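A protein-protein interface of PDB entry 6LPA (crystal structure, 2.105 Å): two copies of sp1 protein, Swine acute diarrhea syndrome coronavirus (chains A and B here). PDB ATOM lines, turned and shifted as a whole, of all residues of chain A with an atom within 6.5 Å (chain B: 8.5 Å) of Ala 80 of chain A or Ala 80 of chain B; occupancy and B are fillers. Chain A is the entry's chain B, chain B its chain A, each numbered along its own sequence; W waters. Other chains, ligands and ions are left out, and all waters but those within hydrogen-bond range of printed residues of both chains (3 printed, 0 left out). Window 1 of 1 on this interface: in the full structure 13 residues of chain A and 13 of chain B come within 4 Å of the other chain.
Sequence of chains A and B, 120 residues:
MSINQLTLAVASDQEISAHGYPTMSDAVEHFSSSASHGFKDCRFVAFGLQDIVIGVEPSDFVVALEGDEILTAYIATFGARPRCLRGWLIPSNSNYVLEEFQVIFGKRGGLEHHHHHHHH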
ATOM      1  N   PHE A  47      -7.468   6.484   5.622  1.00  0.00           N
ATOM      2  CA  PHE A  47      -7.482   7.449   6.724  1.00  0.00           C
ATOM      3  C   PHE A  47      -7.426   8.881   6.210  1.00  0.00           C
ATOM      4  O   PHE A  47      -8.179   9.746   6.665  1.00  0.00           O
ATOM      5  CB  PHE A  47      -6.311   7.212   7.688  1.00  0.00           C
ATOM      6  CG  PHE A  47      -6.260   8.214   8.820  1.00  0.00           C
ATOM      7  CD1 PHE A  47      -6.953   7.976   9.997  1.00  0.00           C
ATOM      8  CD2 PHE A  47      -5.573   9.424   8.685  1.00  0.00           C
ATOM      9  CE1 PHE A  47      -6.933   8.899  11.041  1.00  0.00           C
ATOM     10  CE2 PHE A  47      -5.553  10.358   9.732  1.00  0.00           C
ATOM     11  CZ  PHE A  47      -6.235  10.090  10.905  1.00  0.00           C
ATOM     12  N   PRO A  58     -19.270   9.569  14.550  1.00  0.00           N
ATOM     13  CA  PRO A  58     -18.077   9.055  15.249  1.00  0.00           C
ATOM     14  C   PRO A  58     -18.379   7.871  16.143  1.00  0.00           C
ATOM     15  O   PRO A  58     -17.489   7.034  16.364  1.00  0.00           O
ATOM     16  CB  PRO A  58     -17.586  10.265  16.057  1.00  0.00           C
ATOM     17  CG  PRO A  58     -18.103  11.450  15.310  1.00  0.00           C
ATOM     18  CD  PRO A  58     -19.418  11.029  14.704  1.00  0.00           C
ATOM     19  N   TYR A  74     -10.605  -5.063  12.302  1.00  0.00           N
ATOM     20  CA  TYR A  74     -11.386  -5.307  13.510  1.00  0.00           C
ATOM     21  C   TYR A  74     -12.502  -4.272  13.575  1.00  0.00           C
ATOM     22  O   TYR A  74     -12.445  -3.241  12.907  1.00  0.00           O
ATOM     23  CB  TYR A  74     -10.504  -5.253  14.762  1.00  0.00           C
ATOM     24  CG  TYR A  74      -9.800  -3.933  14.916  1.00  0.00           C
ATOM     25  CD1 TYR A  74      -8.646  -3.656  14.212  1.00  0.00           C
ATOM     26  CD2 TYR A  74     -10.299  -2.957  15.755  1.00  0.00           C
ATOM     27  CE1 TYR A  74      -8.007  -2.427  14.334  1.00  0.00           C
ATOM     28  CE2 TYR A  74      -9.666  -1.741  15.892  1.00  0.00           C
ATOM     29  CZ  TYR A  74      -8.524  -1.484  15.182  1.00  0.00           C
ATOM     30  OH  TYR A  74      -7.901  -0.270  15.322  1.00  0.00           O
ATOM     31  N   ALA A  76     -14.654  -1.321  15.073  1.00  0.00           N
ATOM     32  CA  ALA A  76     -14.328  -0.168  15.907  1.00  0.00           C
ATOM     33  C   ALA A  76     -15.253   0.969  15.525  1.00  0.00           C
ATOM     34  O   ALA A  76     -15.838   0.968  14.439  1.00  0.00           O
ATOM     35  CB  ALA A  76     -12.867   0.262  15.739  1.00  0.00           C
ATOM     36  N   THR A  77     -15.377   1.948  16.425  1.00  0.00           N
ATOM     37  CA  THR A  77     -16.058   3.179  16.049  1.00  0.00           C
ATOM     38  C   THR A  77     -15.241   3.913  14.990  1.00  0.00           C
ATOM     39  O   THR A  77     -14.010   3.862  14.983  1.00  0.00           O
ATOM     40  CB  THR A  77     -16.300   4.103  17.259  1.00  0.00           C
ATOM     41  OG1 THR A  77     -15.071   4.720  17.685  1.00  0.00           O
ATOM     42  CG2 THR A  77     -16.945   3.336  18.442  1.00  0.00           C
ATOM     43  N   PHE A  78     -15.959   4.588  14.087  1.00  0.00           N
ATOM     44  CA  PHE A  78     -15.356   5.410  13.038  1.00  0.00           C
ATOM     45  C   PHE A  78     -14.495   6.527  13.633  1.00  0.00           C
ATOM     46  O   PHE A  78     -13.465   6.898  13.051  1.00  0.00           O
ATOM     47  CB  PHE A  78     -16.500   5.943  12.146  1.00  0.00           C
ATOM     48  CG  PHE A  78     -16.062   6.693  10.883  1.00  0.00           C
ATOM     49  CD1 PHE A  78     -15.004   6.257  10.094  1.00  0.00           C
ATOM     50  CD2 PHE A  78     -16.762   7.834  10.479  1.00  0.00           C
ATOM     51  CE1 PHE A  78     -14.638   6.972   8.918  1.00  0.00           C
ATOM     52  CE2 PHE A  78     -16.412   8.560   9.315  1.00  0.00           C
ATOM     53  CZ  PHE A  78     -15.348   8.125   8.534  1.00  0.00           C
ATOM     54  N   GLY A  79     -14.855   7.036  14.818  1.00  0.00           N
ATOM     55  CA  GLY A  79     -14.069   8.091  15.446  1.00  0.00           C
ATOM     56  C   GLY A  79     -12.843   7.631  16.219  1.00  0.00           C
ATOM     57  O   GLY A  79     -12.055   8.472  16.667  1.00  0.00           O
ATOM     58  N   ALA A  80     -12.651   6.323  16.392  1.00  0.00           N
ATOM     59  CA  ALA A  80     -11.497   5.848  17.147  1.00  0.00           C
ATOM     60  C   ALA A  80     -10.222   6.096  16.353  1.00  0.00           C
ATOM     61  O   ALA A  80     -10.202   5.949  15.124  1.00  0.00           O
ATOM     62  CB  ALA A  80     -11.633   4.358  17.471  1.00  0.00           C
ATOM     63  N   ARG A  81      -9.152   6.470  17.061  1.00  0.00           N
ATOM     64  CA  ARG A  81      -7.868   6.800  16.442  1.00  0.00           C
ATOM     65  C   ARG A  81      -6.697   6.086  17.130  1.00  0.00           C
ATOM     66  O   ARG A  81      -5.872   6.706  17.806  1.00  0.00           O
ATOM     67  CB  ARG A  81      -7.667   8.313  16.447  1.00  0.00           C
ATOM     68  CG  ARG A  81      -8.742   9.064  15.652  1.00  0.00           C
ATOM     69  CD  ARG A  81      -8.420   9.045  14.157  1.00  0.00           C
ATOM     70  NE  ARG A  81      -9.349   9.847  13.356  1.00  0.00           N
ATOM     71  CZ  ARG A  81     -10.567   9.447  12.994  1.00  0.00           C
ATOM     72  NH1 ARG A  81     -11.015   8.261  13.366  1.00  0.00           N
ATOM     73  NH2 ARG A  81     -11.336  10.228  12.251  1.00  0.00           N
ATOM     74  N   PRO A  82      -6.556   4.789  16.914  1.00  0.00           N
ATOM     75  CA  PRO A  82      -5.299   4.141  17.293  1.00  0.00           C
ATOM     76  C   PRO A  82      -4.181   4.614  16.377  1.00  0.00           C
ATOM     77  O   PRO A  82      -4.412   5.142  15.287  1.00  0.00           O
ATOM     78  CB  PRO A  82      -5.590   2.657  17.089  1.00  0.00           C
ATOM     79  CG  PRO A  82      -6.538   2.660  15.935  1.00  0.00           C
ATOM     80  CD  PRO A  82      -7.389   3.911  16.078  1.00  0.00           C
ATOM     81  N   LEU A  85      -3.616   3.303  12.333  1.00  0.00           N
ATOM     82  CA  LEU A  85      -4.878   3.295  11.591  1.00  0.00           C
ATOM     83  C   LEU A  85      -4.625   3.731  10.156  1.00  0.00           C
ATOM     84  O   LEU A  85      -4.170   4.848   9.914  1.00  0.00           O
ATOM     85  CB  LEU A  85      -5.903   4.231  12.246  1.00  0.00           C
ATOM     86  CG  LEU A  85      -7.284   4.274  11.566  1.00  0.00           C
ATOM     87  CD1 LEU A  85      -7.862   2.862  11.501  1.00  0.00           C
ATOM     88  CD2 LEU A  85      -8.256   5.205  12.286  1.00  0.00           C
ATOM     89  N   TRP A  88     -10.633   2.396   6.786  1.00  0.00           N
ATOM     90  CA  TRP A  88     -11.799   1.663   7.265  1.00  0.00           C
ATOM     91  C   TRP A  88     -12.478   0.958   6.108  1.00  0.00           C
ATOM     92  O   TRP A  88     -12.345   1.350   4.949  1.00  0.00           O
ATOM     93  CB  TRP A  88     -12.863   2.544   7.935  1.00  0.00           C
ATOM     94  CG  TRP A  88     -12.359   3.520   8.926  1.00  0.00           C
ATOM     95  CD1 TRP A  88     -12.369   3.381  10.277  1.00  0.00           C
ATOM     96  CD2 TRP A  88     -11.787   4.811   8.653  1.00  0.00           C
ATOM     97  NE1 TRP A  88     -11.831   4.503  10.867  1.00  0.00           N
ATOM     98  CE2 TRP A  88     -11.467   5.392   9.890  1.00  0.00           C
ATOM     99  CE3 TRP A  88     -11.506   5.521   7.481  1.00  0.00           C
ATOM    100  CZ2 TRP A  88     -10.885   6.659   9.994  1.00  0.00           C
ATOM    101  CZ3 TRP A  88     -10.940   6.764   7.581  1.00  0.00           C
ATOM    102  CH2 TRP A  88     -10.631   7.329   8.829  1.00  0.00           C
ATOM    103  N   PHE B  47     -17.460   4.711  32.988  1.00  0.00           N
ATOM    104  CA  PHE B  47     -17.481   5.872  32.115  1.00  0.00           C
ATOM    105  C   PHE B  47     -17.875   7.096  32.929  1.00  0.00           C
ATOM    106  O   PHE B  47     -18.835   7.055  33.708  1.00  0.00           O
ATOM    107  CB  PHE B  47     -18.458   5.686  30.959  1.00  0.00           C
ATOM    108  CG  PHE B  47     -18.524   6.888  30.049  1.00  0.00           C
ATOM    109  CD1 PHE B  47     -17.568   7.071  29.055  1.00  0.00           C
ATOM    110  CD2 PHE B  47     -19.484   7.878  30.243  1.00  0.00           C
ATOM    111  CE1 PHE B  47     -17.581   8.187  28.234  1.00  0.00           C
ATOM    112  CE2 PHE B  47     -19.527   8.983  29.411  1.00  0.00           C
ATOM    113  CZ  PHE B  47     -18.556   9.148  28.403  1.00  0.00           C
ATOM    114  N   GLN B  50     -12.857   8.522  33.523  1.00  0.00           N
ATOM    115  CA  GLN B  50     -11.608   8.364  32.790  1.00  0.00           C
ATOM    116  C   GLN B  50     -10.583   9.399  33.203  1.00  0.00           C
ATOM    117  O   GLN B  50      -9.383   9.176  33.021  1.00  0.00           O
ATOM    118  CB  GLN B  50     -11.839   8.435  31.271  1.00  0.00           C
ATOM    119  CG  GLN B  50     -12.482   9.727  30.789  1.00  0.00           C
ATOM    120  CD  GLN B  50     -13.986   9.609  30.741  1.00  0.00           C
ATOM    121  OE1 GLN B  50     -14.566   8.747  31.406  1.00  0.00           O
ATOM    122  NE2 GLN B  50     -14.631  10.459  29.946  1.00  0.00           N
ATOM    123  N   GLU B  57      -3.310   6.595  26.967  1.00  0.00           N
ATOM    124  CA  GLU B  57      -3.592   7.550  25.906  1.00  0.00           C
ATOM    125  C   GLU B  57      -4.903   7.205  25.210  1.00  0.00           C
ATOM    126  O   GLU B  57      -5.327   6.039  25.206  1.00  0.00           O
ATOM    127  CB  GLU B  57      -2.461   7.538  24.879  1.00  0.00           C
ATOM    128  CG  GLU B  57      -1.958   8.898  24.475  1.00  0.00           C
ATOM    129  CD  GLU B  57      -1.211   9.573  25.595  1.00  0.00           C
ATOM    130  OE1 GLU B  57      -0.044   9.200  25.821  1.00  0.00           O
ATOM    131  OE2 GLU B  57      -1.786  10.467  26.248  1.00  0.00           O
ATOM    132  N   PRO B  58      -5.555   8.198  24.585  1.00  0.00           N
ATOM    133  CA  PRO B  58      -6.775   7.898  23.819  1.00  0.00           C
ATOM    134  C   PRO B  58      -6.564   6.856  22.728  1.00  0.00           C
ATOM    135  O   PRO B  58      -7.490   6.098  22.412  1.00  0.00           O
ATOM    136  CB  PRO B  58      -7.160   9.270  23.238  1.00  0.00           C
ATOM    137  CG  PRO B  58      -6.583  10.240  24.184  1.00  0.00           C
ATOM    138  CD  PRO B  58      -5.299   9.651  24.654  1.00  0.00           C
ATOM    139  N   SER B  59      -5.366   6.782  22.153  1.00  0.00           N
ATOM    140  CA  SER B  59      -5.071   5.778  21.138  1.00  0.00           C
ATOM    141  C   SER B  59      -4.783   4.398  21.722  1.00  0.00           C
ATOM    142  O   SER B  59      -4.709   3.424  20.964  1.00  0.00           O
ATOM    143  CB  SER B  59      -3.871   6.234  20.315  1.00  0.00           C
ATOM    144  OG  SER B  59      -2.819   6.576  21.195  1.00  0.00           O
ATOM    145  N   ASP B  60      -4.605   4.282  23.034  1.00  0.00           N
ATOM    146  CA  ASP B  60      -4.227   2.996  23.613  1.00  0.00           C
ATOM    147  C   ASP B  60      -5.420   2.051  23.648  1.00  0.00           C
ATOM    148  O   ASP B  60      -6.548   2.455  23.938  1.00  0.00           O
ATOM    149  CB  ASP B  60      -3.669   3.191  25.023  1.00  0.00           C
ATOM    150  CG  ASP B  60      -2.248   3.732  25.012  1.00  0.00           C
ATOM    151  OD1 ASP B  60      -1.501   3.396  24.071  1.00  0.00           O
ATOM    152  OD2 ASP B  60      -1.896   4.514  25.922  1.00  0.00           O
ATOM    153  N   PHE B  61      -5.162   0.784  23.366  1.00  0.00           N
ATOM    154  CA  PHE B  61      -6.205  -0.225  23.403  1.00  0.00           C
ATOM    155  C   PHE B  61      -6.421  -0.722  24.825  1.00  0.00           C
ATOM    156  O   PHE B  61      -5.469  -1.079  25.527  1.00  0.00           O
ATOM    157  CB  PHE B  61      -5.847  -1.391  22.487  1.00  0.00           C
ATOM    158  CG  PHE B  61      -6.081  -1.089  21.047  1.00  0.00           C
ATOM    159  CD1 PHE B  61      -7.369  -1.078  20.534  1.00  0.00           C
ATOM    160  CD2 PHE B  61      -5.025  -0.763  20.216  1.00  0.00           C
ATOM    161  CE1 PHE B  61      -7.589  -0.777  19.200  1.00  0.00           C
ATOM    162  CE2 PHE B  61      -5.244  -0.454  18.883  1.00  0.00           C
ATOM    163  CZ  PHE B  61      -6.523  -0.472  18.376  1.00  0.00           C
ATOM    164  N   VAL B  62      -7.679  -0.720  25.249  1.00  0.00           N
ATOM    165  CA  VAL B  62      -8.095  -1.328  26.507  1.00  0.00           C
ATOM    166  C   VAL B  62      -9.282  -2.233  26.192  1.00  0.00           C
ATOM    167  O   VAL B  62      -9.619  -2.430  25.016  1.00  0.00           O
ATOM    168  CB  VAL B  62      -8.432  -0.244  27.550  1.00  0.00           C
ATOM    169  CG1 VAL B  62      -7.214   0.646  27.807  1.00  0.00           C
ATOM    170  CG2 VAL B  62      -9.561   0.620  27.067  1.00  0.00           C
ATOM    171  N   ALA B  64     -13.242  -2.418  26.456  1.00  0.00           N
ATOM    172  CA  ALA B  64     -14.421  -1.592  26.661  1.00  0.00           C
ATOM    173  C   ALA B  64     -15.600  -2.498  26.991  1.00  0.00           C
ATOM    174  O   ALA B  64     -15.615  -3.675  26.631  1.00  0.00           O
ATOM    175  CB  ALA B  64     -14.734  -0.739  25.422  1.00  0.00           C
ATOM    176  N   GLU B  66     -19.881  -2.216  26.909  1.00  0.00           N
ATOM    177  CA  GLU B  66     -21.079  -1.464  26.565  1.00  0.00           C
ATOM    178  C   GLU B  66     -22.305  -2.344  26.760  1.00  0.00           C
ATOM    179  O   GLU B  66     -22.220  -3.574  26.664  1.00  0.00           O
ATOM    180  CB  GLU B  66     -21.043  -0.963  25.122  1.00  0.00           C
ATOM    181  CG  GLU B  66     -21.222  -2.029  24.070  1.00  0.00           C
ATOM    182  CD  GLU B  66     -21.102  -1.458  22.658  1.00  0.00           C
ATOM    183  OE1 GLU B  66     -21.972  -1.760  21.809  1.00  0.00           O
ATOM    184  OE2 GLU B  66     -20.137  -0.697  22.409  1.00  0.00           O
ATOM    185  N   TYR B  74     -15.154  -5.879  24.678  1.00  0.00           N
ATOM    186  CA  TYR B  74     -14.383  -6.014  23.449  1.00  0.00           C
ATOM    187  C   TYR B  74     -13.190  -5.085  23.552  1.00  0.00           C
ATOM    188  O   TYR B  74     -13.143  -4.205  24.411  1.00  0.00           O
ATOM    189  CB  TYR B  74     -15.230  -5.689  22.217  1.00  0.00           C
ATOM    190  CG  TYR B  74     -15.865  -4.313  22.265  1.00  0.00           C
ATOM    191  CD1 TYR B  74     -17.035  -4.095  22.984  1.00  0.00           C
ATOM    192  CD2 TYR B  74     -15.309  -3.240  21.584  1.00  0.00           C
ATOM    193  CE1 TYR B  74     -17.621  -2.852  23.037  1.00  0.00           C
ATOM    194  CE2 TYR B  74     -15.892  -1.974  21.634  1.00  0.00           C
ATOM    195  CZ  TYR B  74     -17.049  -1.792  22.356  1.00  0.00           C
ATOM    196  OH  TYR B  74     -17.649  -0.554  22.423  1.00  0.00           O
ATOM    197  N   ILE B  75     -12.232  -5.284  22.669  1.00  0.00           N
ATOM    198  CA  ILE B  75     -11.025  -4.468  22.651  1.00  0.00           C
ATOM    199  C   ILE B  75     -11.292  -3.225  21.817  1.00  0.00           C
ATOM    200  O   ILE B  75     -11.877  -3.304  20.734  1.00  0.00           O
ATOM    201  CB  ILE B  75      -9.831  -5.283  22.119  1.00  0.00           C
ATOM    202  CG1 ILE B  75      -9.586  -6.461  23.042  1.00  0.00           C
ATOM    203  CG2 ILE B  75      -8.576  -4.424  22.031  1.00  0.00           C
ATOM    204  CD1 ILE B  75      -8.377  -7.319  22.655  1.00  0.00           C
ATOM    205  N   ALA B  76     -10.895  -2.070  22.345  1.00  0.00           N
ATOM    206  CA  ALA B  76     -11.175  -0.764  21.757  1.00  0.00           C
ATOM    207  C   ALA B  76     -10.185   0.245  22.327  1.00  0.00           C
ATOM    208  O   ALA B  76      -9.598   0.025  23.394  1.00  0.00           O
ATOM    209  CB  ALA B  76     -12.624  -0.321  22.030  1.00  0.00           C
ATOM    210  N   THR B  77      -9.980   1.347  21.600  1.00  0.00           N
ATOM    211  CA  THR B  77      -9.144   2.409  22.143  1.00  0.00           C
ATOM    212  C   THR B  77      -9.837   3.048  23.336  1.00  0.00           C
ATOM    213  O   THR B  77     -11.068   3.129  23.389  1.00  0.00           O
ATOM    214  CB  THR B  77      -8.840   3.500  21.098  1.00  0.00           C
ATOM    215  OG1 THR B  77     -10.066   4.084  20.623  1.00  0.00           O
ATOM    216  CG2 THR B  77      -8.022   2.922  19.913  1.00  0.00           C
ATOM    217  N   PHE B  78      -9.021   3.539  24.279  1.00  0.00           N
ATOM    218  CA  PHE B  78      -9.543   4.203  25.470  1.00  0.00           C
ATOM    219  C   PHE B  78     -10.380   5.420  25.091  1.00  0.00           C
ATOM    220  O   PHE B  78     -11.365   5.742  25.771  1.00  0.00           O
ATOM    221  CB  PHE B  78      -8.362   4.577  26.384  1.00  0.00           C
ATOM    222  CG  PHE B  78      -8.746   5.118  27.744  1.00  0.00           C
ATOM    223  CD1 PHE B  78      -9.846   4.620  28.452  1.00  0.00           C
ATOM    224  CD2 PHE B  78      -7.970   6.114  28.339  1.00  0.00           C
ATOM    225  CE1 PHE B  78     -10.181   5.146  29.726  1.00  0.00           C
ATOM    226  CE2 PHE B  78      -8.289   6.631  29.585  1.00  0.00           C
ATOM    227  CZ  PHE B  78      -9.395   6.142  30.290  1.00  0.00           C
ATOM    228  N   GLY B  79     -10.026   6.082  23.981  1.00  0.00           N
ATOM    229  CA  GLY B  79     -10.728   7.264  23.515  1.00  0.00           C
ATOM    230  C   GLY B  79     -11.994   7.007  22.709  1.00  0.00           C
ATOM    231  O   GLY B  79     -12.777   7.938  22.505  1.00  0.00           O
ATOM    232  N   ALA B  80     -12.232   5.778  22.261  1.00  0.00           N
ATOM    233  CA  ALA B  80     -13.450   5.520  21.497  1.00  0.00           C
ATOM    234  C   ALA B  80     -14.698   5.768  22.344  1.00  0.00           C
ATOM    235  O   ALA B  80     -14.715   5.536  23.558  1.00  0.00           O
ATOM    236  CB  ALA B  80     -13.466   4.087  20.961  1.00  0.00           C
ATOM    237  N   ARG B  81     -15.757   6.233  21.683  1.00  0.00           N
ATOM    238  CA  ARG B  81     -16.998   6.638  22.345  1.00  0.00           C
ATOM    239  C   ARG B  81     -18.221   6.091  21.611  1.00  0.00           C
ATOM    240  O   ARG B  81     -18.957   6.841  20.958  1.00  0.00           O
ATOM    241  CB  ARG B  81     -17.080   8.163  22.450  1.00  0.00           C
ATOM    242  CG  ARG B  81     -16.041   8.797  23.357  1.00  0.00           C
ATOM    243  CD  ARG B  81     -16.385   8.564  24.820  1.00  0.00           C
ATOM    244  NE  ARG B  81     -15.402   9.171  25.713  1.00  0.00           N
ATOM    245  CZ  ARG B  81     -14.214   8.647  25.985  1.00  0.00           C
ATOM    246  NH1 ARG B  81     -13.845   7.491  25.442  1.00  0.00           N
ATOM    247  NH2 ARG B  81     -13.391   9.275  26.807  1.00  0.00           N
ATOM    248  N   PRO B  82     -18.503   4.795  21.735  1.00  0.00           N
ATOM    249  CA  PRO B  82     -19.791   4.283  21.272  1.00  0.00           C
ATOM    250  C   PRO B  82     -20.886   4.619  22.270  1.00  0.00           C
ATOM    251  O   PRO B  82     -20.642   4.904  23.450  1.00  0.00           O
ATOM    252  CB  PRO B  82     -19.571   2.773  21.198  1.00  0.00           C
ATOM    253  CG  PRO B  82     -18.624   2.522  22.311  1.00  0.00           C
ATOM    254  CD  PRO B  82     -17.711   3.739  22.389  1.00  0.00           C
ATOM    255  N   ARG B  83     -22.118   4.586  21.778  1.00  0.00           N
ATOM    256  CA  ARG B  83     -23.250   4.744  22.672  1.00  0.00           C
ATOM    257  C   ARG B  83     -23.289   3.579  23.657  1.00  0.00           C
ATOM    258  O   ARG B  83     -22.825   2.471  23.364  1.00  0.00           O
ATOM    259  CB  ARG B  83     -24.558   4.819  21.884  1.00  0.00           C
ATOM    260  CG  ARG B  83     -24.542   5.814  20.731  1.00  0.00           C
ATOM    261  CD  ARG B  83     -25.460   5.337  19.597  1.00  0.00           C
ATOM    262  NE  ARG B  83     -25.528   6.255  18.454  1.00  0.00           N
ATOM    263  CZ  ARG B  83     -25.072   5.977  17.230  1.00  0.00           C
ATOM    264  NH1 ARG B  83     -24.484   4.812  16.977  1.00  0.00           N
ATOM    265  NH2 ARG B  83     -25.195   6.871  16.256  1.00  0.00           N
ATOM    266  N   LEU B  85     -21.522   3.060  26.120  1.00  0.00           N
ATOM    267  CA  LEU B  85     -20.254   2.731  26.758  1.00  0.00           C
ATOM    268  C   LEU B  85     -20.403   2.897  28.269  1.00  0.00           C
ATOM    269  O   LEU B  85     -20.745   3.977  28.754  1.00  0.00           O
ATOM    270  CB  LEU B  85     -19.133   3.624  26.218  1.00  0.00           C
ATOM    271  CG  LEU B  85     -17.769   3.459  26.896  1.00  0.00           C
ATOM    272  CD1 LEU B  85     -17.274   2.008  26.749  1.00  0.00           C
ATOM    273  CD2 LEU B  85     -16.755   4.423  26.300  1.00  0.00           C
ATOM    274  N   GLY B  87     -17.900   1.612  30.589  1.00  0.00           N
ATOM    275  CA  GLY B  87     -16.635   1.668  31.278  1.00  0.00           C
ATOM    276  C   GLY B  87     -15.628   0.758  30.606  1.00  0.00           C
ATOM    277  O   GLY B  87     -15.880   0.213  29.536  1.00  0.00           O
ATOM    278  N   TRP B  88     -14.478   0.623  31.260  1.00  0.00           N
ATOM    279  CA  TRP B  88     -13.371  -0.135  30.695  1.00  0.00           C
ATOM    280  C   TRP B  88     -12.754  -1.029  31.760  1.00  0.00           C
ATOM    281  O   TRP B  88     -12.845  -0.759  32.959  1.00  0.00           O
ATOM    282  CB  TRP B  88     -12.270   0.772  30.139  1.00  0.00           C
ATOM    283  CG  TRP B  88     -12.722   1.878  29.230  1.00  0.00           C
ATOM    284  CD1 TRP B  88     -12.732   1.864  27.863  1.00  0.00           C
ATOM    285  CD2 TRP B  88     -13.187   3.183  29.628  1.00  0.00           C
ATOM    286  NE1 TRP B  88     -13.184   3.087  27.386  1.00  0.00           N
ATOM    287  CE2 TRP B  88     -13.475   3.907  28.445  1.00  0.00           C
ATOM    288  CE3 TRP B  88     -13.396   3.803  30.866  1.00  0.00           C
ATOM    289  CZ2 TRP B  88     -13.967   5.222  28.468  1.00  0.00           C
ATOM    290  CZ3 TRP B  88     -13.896   5.117  30.889  1.00  0.00           C
ATOM    291  CH2 TRP B  88     -14.161   5.814  29.693  1.00  0.00           C
HETATM  292  O   HOH W   1     -15.461   7.123  18.819  1.00  0.00           O
HETATM  293  O   HOH W   2     -13.601   9.226  19.594  1.00  0.00           O
HETATM  294  O   HOH W   3      -9.523   6.669  20.043  1.00  0.00           O
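Water W1 lies within hydrogen-bond range of the side-chain hydroxyl (OG1) of Thr 77 of chain A, the backbone NH (N) of Arg 81 of chain B and the backbone carbonyl oxygen (O) of Pro 58 of chain A. Water W3 lies within hydrogen-bond range of OG1 of Thr 77 of chain B (2.7 Å), N of Arg 81 of chain A (3.0 Å) and O of Pro 58 of chain B (3.2 Å). Water W2 bridges O of Gly 79 of chain B (3.3 Å) and O of Gly 79 of chain A (3.4 Å).
Printed residues of chain B within 4 Å of Tyr 74 of chain A: Phe 61 (3.4 Å). Phe 78 of chain A touches none of the printed residues of chain B. No residue of chain B comes within 4 Å of Gly 79 of chain A. Ala 80 of chain A touches just these residues of chain B: Thr 77 (3.5 Å) and Ala 80 (3.95 Å). Of chain A, only Thr 77 and Ala 80 come within 4 Å of Ala 80 of chain B. Of the printed residues of chain A, Pro 82 of chain B touches Thr 77. The nearest residue of chain A that does not touch Ala 80 of chain B is Gly 79 of chain A (5.7 Å). The nearest printed residue of chain B that does not touch Thr 77 of chain A is Arg 81 of chain B (4.3 Å).
Among the printed residues, pairs that only touch across the chains: Tyr 74 of chain A with Phe 61 of chain B (3.4 Å), Thr 77 of chain A with Ala 80 of chain B (3.7 Å), Thr 77 of chain A with Pro 82 of chain B (3.8 Å), Ala 80 of chain A with Thr 77 of chain B (3.5 Å), Ala 80 of chain A with Ala 80 of chain B (3.95 Å), Arg 81 of chain A with Ser 59 of chain B (3.2 Å), Pro 82 of chain A with Ser 59 of chain B (3.8 Å), Pro 82 of chain A with Phe 61 of chain B (3.5 Å) and Pro 82 of chain A with Thr 77 of chain B (3.7 Å).
The backbone carbonyl oxygen (O) of Gly 79 of chain A sits close to the guanidinium group (NH1) of Arg 81 of chain A (3.5 Å). The side-chain hydroxyl of Thr 77 of chain B sits at hydrogen-bond distance from the backbone NH of Ala 80 of chain B (3.2 Å). The side-chain hydroxyl (OG1) of Thr 77 of chain A is in hydrogen-bond range of the backbone NH (N) of Ala 80 of chain A (3.2 Å). O of Phe 78 of chain A sits at hydrogen-bond distance from NH1 of Arg 81 of chain A (2.8 Å).
Thr 77 of chain A touches Ala 80 of chain B, and with the chains exchanged Ala 80 of chain A touches Thr 77 of chain B. Thr 77 of chain A touches Pro 82 of chain B, and with the chains exchanged Pro 82 of chain A touches Thr 77 of chain B. Ala 80 of chain A touches its own counterpart, Ala 80 of chain B. Positions printed for both chains: 47, 58, 74, 76, 77, 78, 79, 80, 81, 82, 85 and 88. Of the 9 pairs that touch across the chains among the printed residues, 5 have their exchanged pair printed and touching as well.
Of the 23 printed residues of chain B, 5 touch a printed residue of chain A. Of the 12 printed residues of chain A, 5 touch a printed residue of chain B. Hydrophobic or aromatic side chains of chain A within 4 Å of the printed part of chain B: Tyr 74, Ala 80 and Pro 82.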
